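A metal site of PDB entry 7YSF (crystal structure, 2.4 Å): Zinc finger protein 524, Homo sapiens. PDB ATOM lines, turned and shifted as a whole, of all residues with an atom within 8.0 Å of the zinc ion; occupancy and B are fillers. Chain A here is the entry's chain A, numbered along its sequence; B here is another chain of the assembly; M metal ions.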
ATOM      1  N   GLN A  39      -2.249 -17.353  13.543  1.00  0.00           N
ATOM      2  CA  GLN A  39      -2.795 -16.370  14.462  1.00  0.00           C
ATOM      3  C   GLN A  39      -1.702 -15.365  14.813  1.00  0.00           C
ATOM      4  O   GLN A  39      -0.589 -15.753  15.180  1.00  0.00           O
ATOM      5  CB  GLN A  39      -3.330 -17.028  15.737  1.00  0.00           C
ATOM      6  CG  GLN A  39      -3.801 -16.036  16.805  1.00  0.00           C
ATOM      7  CD  GLN A  39      -4.488 -16.713  17.975  1.00  0.00           C
ATOM      8  OE1 GLN A  39      -4.010 -17.718  18.509  1.00  0.00           O
ATOM      9  NE2 GLN A  39      -5.623 -16.166  18.387  1.00  0.00           N
ATOM     10  N   CYS A  40      -2.026 -14.076  14.685  1.00  0.00           N
ATOM     11  CA  CYS A  40      -1.147 -13.005  15.136  1.00  0.00           C
ATOM     12  C   CYS A  40      -1.256 -12.870  16.650  1.00  0.00           C
ATOM     13  O   CYS A  40      -2.322 -12.520  17.168  1.00  0.00           O
ATOM     14  CB  CYS A  40      -1.540 -11.700  14.442  1.00  0.00           C
ATOM     15  SG  CYS A  40      -0.694 -10.211  15.040  1.00  0.00           S
ATOM     16  N   LYS A  41      -0.157 -13.116  17.358  1.00  0.00           N
ATOM     17  CA  LYS A  41      -0.192 -13.035  18.807  1.00  0.00           C
ATOM     18  C   LYS A  41      -0.126 -11.599  19.326  1.00  0.00           C
ATOM     19  O   LYS A  41      -0.066 -11.414  20.548  1.00  0.00           O
ATOM     20  CB  LYS A  41       0.946 -13.864  19.423  1.00  0.00           C
ATOM     21  CG  LYS A  41       0.936 -15.326  18.966  1.00  0.00           C
ATOM     22  CD  LYS A  41       0.351 -16.238  20.041  1.00  0.00           C
ATOM     23  CE  LYS A  41      -0.345 -17.427  19.414  1.00  0.00           C
ATOM     24  NZ  LYS A  41       0.018 -18.697  20.073  1.00  0.00           N
ATOM     25  N   VAL A  42      -0.115 -10.602  18.443  1.00  0.00           N
ATOM     26  CA  VAL A  42      -0.221  -9.207  18.859  1.00  0.00           C
ATOM     27  C   VAL A  42      -1.671  -8.813  19.098  1.00  0.00           C
ATOM     28  O   VAL A  42      -2.011  -8.263  20.154  1.00  0.00           O
ATOM     29  CB  VAL A  42       0.447  -8.295  17.799  1.00  0.00           C
ATOM     30  CG1 VAL A  42       0.166  -6.835  18.115  1.00  0.00           C
ATOM     31  CG2 VAL A  42       1.932  -8.571  17.708  1.00  0.00           C
ATOM     32  N   CYS A  43      -2.546  -9.060  18.128  1.00  0.00           N
ATOM     33  CA  CYS A  43      -3.938  -8.654  18.215  1.00  0.00           C
ATOM     34  C   CYS A  43      -4.933  -9.807  18.260  1.00  0.00           C
ATOM     35  O   CYS A  43      -6.091  -9.580  18.628  1.00  0.00           O
ATOM     36  CB  CYS A  43      -4.308  -7.733  17.042  1.00  0.00           C
ATOM     37  SG  CYS A  43      -4.400  -8.567  15.435  1.00  0.00           S
ATOM     38  N   GLY A  44      -4.522 -11.017  17.887  1.00  0.00           N
ATOM     39  CA  GLY A  44      -5.358 -12.199  18.005  1.00  0.00           C
ATOM     40  C   GLY A  44      -5.997 -12.673  16.714  1.00  0.00           C
ATOM     41  O   GLY A  44      -6.471 -13.806  16.659  1.00  0.00           O
ATOM     42  N   LYS A  45      -6.024 -11.831  15.682  1.00  0.00           N
ATOM     43  CA  LYS A  45      -6.709 -12.198  14.443  1.00  0.00           C
ATOM     44  C   LYS A  45      -6.039 -13.393  13.782  1.00  0.00           C
ATOM     45  O   LYS A  45      -4.818 -13.535  13.790  1.00  0.00           O
ATOM     46  CB  LYS A  45      -6.738 -11.011  13.490  1.00  0.00           C
ATOM     47  CG  LYS A  45      -7.595  -9.842  13.969  1.00  0.00           C
ATOM     48  CD  LYS A  45      -7.269  -8.570  13.201  1.00  0.00           C
ATOM     49  CE  LYS A  45      -8.243  -7.451  13.558  1.00  0.00           C
ATOM     50  NZ  LYS A  45      -9.336  -7.334  12.552  1.00  0.00           N
ATOM     51  N   THR A  46      -6.870 -14.262  13.195  1.00  0.00           N
ATOM     52  CA  THR A  46      -6.398 -15.454  12.518  1.00  0.00           C
ATOM     53  C   THR A  46      -6.402 -15.252  11.011  1.00  0.00           C
ATOM     54  O   THR A  46      -7.125 -14.399  10.475  1.00  0.00           O
ATOM     55  CB  THR A  46      -7.259 -16.678  12.883  1.00  0.00           C
ATOM     56  OG1 THR A  46      -8.563 -16.535  12.300  1.00  0.00           O
ATOM     57  CG2 THR A  46      -7.391 -16.808  14.395  1.00  0.00           C
ATOM     58  N   PHE A  47      -5.591 -16.048  10.324  1.00  0.00           N
ATOM     59  CA  PHE A  47      -5.379 -15.870   8.890  1.00  0.00           C
ATOM     60  C   PHE A  47      -5.276 -17.218   8.192  1.00  0.00           C
ATOM     61  O   PHE A  47      -4.887 -18.221   8.792  1.00  0.00           O
ATOM     62  CB  PHE A  47      -4.122 -15.030   8.621  1.00  0.00           C
ATOM     63  CG  PHE A  47      -4.232 -13.633   9.139  1.00  0.00           C
ATOM     64  CD1 PHE A  47      -4.795 -12.626   8.366  1.00  0.00           C
ATOM     65  CD2 PHE A  47      -3.808 -13.322  10.422  1.00  0.00           C
ATOM     66  CE1 PHE A  47      -4.919 -11.350   8.853  1.00  0.00           C
ATOM     67  CE2 PHE A  47      -3.930 -12.045  10.919  1.00  0.00           C
ATOM     68  CZ  PHE A  47      -4.495 -11.053  10.126  1.00  0.00           C
ATOM     69  N   LEU A  53      -0.681 -13.549   7.135  1.00  0.00           N
ATOM     70  CA  LEU A  53      -0.211 -13.179   8.473  1.00  0.00           C
ATOM     71  C   LEU A  53       0.998 -12.253   8.396  1.00  0.00           C
ATOM     72  O   LEU A  53       1.067 -11.258   9.118  1.00  0.00           O
ATOM     73  CB  LEU A  53       0.131 -14.443   9.268  1.00  0.00           C
ATOM     74  CG  LEU A  53       0.789 -14.183  10.622  1.00  0.00           C
ATOM     75  CD1 LEU A  53      -0.186 -13.471  11.558  1.00  0.00           C
ATOM     76  CD2 LEU A  53       1.293 -15.481  11.246  1.00  0.00           C
ATOM     77  N   HIS A  56      -0.073  -8.917   7.318  1.00  0.00           N
ATOM     78  CA  HIS A  56      -0.784  -8.270   8.410  1.00  0.00           C
ATOM     79  C   HIS A  56       0.157  -7.815   9.516  1.00  0.00           C
ATOM     80  O   HIS A  56      -0.092  -6.792  10.171  1.00  0.00           O
ATOM     81  CB  HIS A  56      -1.843  -9.208   8.978  1.00  0.00           C
ATOM     82  CG  HIS A  56      -2.310  -8.840  10.356  1.00  0.00           C
ATOM     83  ND1 HIS A  56      -3.408  -8.048  10.585  1.00  0.00           N
ATOM     84  CD2 HIS A  56      -1.816  -9.160  11.573  1.00  0.00           C
ATOM     85  CE1 HIS A  56      -3.577  -7.889  11.887  1.00  0.00           C
ATOM     86  NE2 HIS A  56      -2.622  -8.559  12.508  1.00  0.00           N
ATOM     87  N   CYS A  57       1.241  -8.556   9.748  1.00  0.00           N
ATOM     88  CA  CYS A  57       2.195  -8.183  10.789  1.00  0.00           C
ATOM     89  C   CYS A  57       2.789  -6.798  10.525  1.00  0.00           C
ATOM     90  O   CYS A  57       3.165  -6.102  11.470  1.00  0.00           O
ATOM     91  CB  CYS A  57       3.314  -9.228  10.866  1.00  0.00           C
ATOM     92  SG  CYS A  57       4.063  -9.432  12.508  1.00  0.00           S
ATOM     93  N   ASN A  58       2.883  -6.404   9.249  1.00  0.00           N
ATOM     94  CA  ASN A  58       3.424  -5.100   8.921  1.00  0.00           C
ATOM     95  C   ASN A  58       2.570  -3.962   9.480  1.00  0.00           C
ATOM     96  O   ASN A  58       3.084  -2.877   9.741  1.00  0.00           O
ATOM     97  CB  ASN A  58       3.559  -4.948   7.398  1.00  0.00           C
ATOM     98  CG  ASN A  58       4.563  -5.912   6.807  1.00  0.00           C
ATOM     99  OD1 ASN A  58       5.536  -6.297   7.452  1.00  0.00           O
ATOM    100  ND2 ASN A  58       4.345  -6.296   5.546  1.00  0.00           N
ATOM    101  N   ILE A  59       1.264  -4.206   9.660  1.00  0.00           N
ATOM    102  CA  ILE A  59       0.375  -3.153  10.133  1.00  0.00           C
ATOM    103  C   ILE A  59       0.790  -2.670  11.513  1.00  0.00           C
ATOM    104  O   ILE A  59       0.791  -1.465  11.804  1.00  0.00           O
ATOM    105  CB  ILE A  59      -1.087  -3.654  10.131  1.00  0.00           C
ATOM    106  CG1 ILE A  59      -1.591  -3.803   8.692  1.00  0.00           C
ATOM    107  CG2 ILE A  59      -1.980  -2.706  10.896  1.00  0.00           C
ATOM    108  CD1 ILE A  59      -2.796  -4.706   8.555  1.00  0.00           C
ATOM    109  N   HIS A  60       1.190  -3.597  12.397  1.00  0.00           N
ATOM    110  CA  HIS A  60       1.539  -3.254  13.766  1.00  0.00           C
ATOM    111  C   HIS A  60       2.820  -2.428  13.878  1.00  0.00           C
ATOM    112  O   HIS A  60       3.165  -1.997  14.985  1.00  0.00           O
ATOM    113  CB  HIS A  60       1.666  -4.520  14.608  1.00  0.00           C
ATOM    114  CG  HIS A  60       0.384  -5.278  14.742  1.00  0.00           C
ATOM    115  ND1 HIS A  60      -0.806  -4.670  15.074  1.00  0.00           N
ATOM    116  CD2 HIS A  60       0.100  -6.587  14.589  1.00  0.00           C
ATOM    117  CE1 HIS A  60      -1.764  -5.570  15.118  1.00  0.00           C
ATOM    118  NE2 HIS A  60      -1.242  -6.744  14.828  1.00  0.00           N
ATOM    119  P    DG B   8      -6.364  -7.860   8.513  1.00  0.00           P
ATOM    120  OP1  DG B   8      -6.781  -8.429   9.810  1.00  0.00           O
ATOM    121  OP2  DG B   8      -4.937  -7.552   8.272  1.00  0.00           O
ATOM    122  O5'  DG B   8      -6.897  -8.827   7.365  1.00  0.00           O
ATOM    123  C5'  DG B   8      -8.279  -9.125   7.323  1.00  0.00           C
ATOM    124  C4'  DG B   8      -8.696  -9.631   5.963  1.00  0.00           C
ATOM    125  O4'  DG B   8      -8.255  -8.701   4.943  1.00  0.00           O
ATOM    126  C3'  DG B   8      -8.138 -10.989   5.561  1.00  0.00           C
ATOM    127  O3'  DG B   8      -9.218 -11.859   5.241  1.00  0.00           O
ATOM    128  C2'  DG B   8      -7.262 -10.690   4.330  1.00  0.00           C
ATOM    129  C1'  DG B   8      -7.933  -9.441   3.794  1.00  0.00           C
ATOM    130  N9   DG B   8      -7.091  -8.605   2.947  1.00  0.00           N
ATOM    131  C8   DG B   8      -5.932  -7.950   3.299  1.00  0.00           C
ATOM    132  N7   DG B   8      -5.424  -7.249   2.313  1.00  0.00           N
ATOM    133  C5   DG B   8      -6.311  -7.444   1.265  1.00  0.00           C
ATOM    134  C6   DG B   8      -6.282  -6.940  -0.069  1.00  0.00           C
ATOM    135  O6   DG B   8      -5.439  -6.196  -0.584  1.00  0.00           O
ATOM    136  N1   DG B   8      -7.372  -7.388  -0.814  1.00  0.00           N
ATOM    137  C2   DG B   8      -8.357  -8.216  -0.337  1.00  0.00           C
ATOM    138  N2   DG B   8      -9.330  -8.540  -1.212  1.00  0.00           N
ATOM    139  N3   DG B   8      -8.398  -8.696   0.897  1.00  0.00           N
ATOM    140  C4   DG B   8      -7.343  -8.272   1.638  1.00  0.00           C
HETATM  141 ZN    ZN M   1      -2.200  -8.556  14.557  1.00  0.00          ZN
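Within 4 Å of the zinc ion: Cys 40, Cys 43, His 56 and His 60.
The zinc ion is bound by a ring nitrogen (NE2) of His 60, a ring nitrogen (NE2) of His 56, the side-chain sulfur of Cys 40 and the side-chain sulfur of Cys 43. The zinc ion has four donor atoms within binding distance.
OP2 of DG 8 of chain B is in hydrogen-bond range of a ring nitrogen (ND1) of His 56 (2.8 Å). The side-chain sulfur (SG) of Cys 40 sits close to the backbone NH (N) of Val 42, 3.5 Å away. The backbone carbonyl oxygen (O) of Lys 45 is in hydrogen-bond range of the backbone NH (N) of Cys 40 (3.0 Å). The side-chain sulfur (SG) of Cys 43 sits close to the backbone NH (N) of Lys 45 (3.7 Å).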
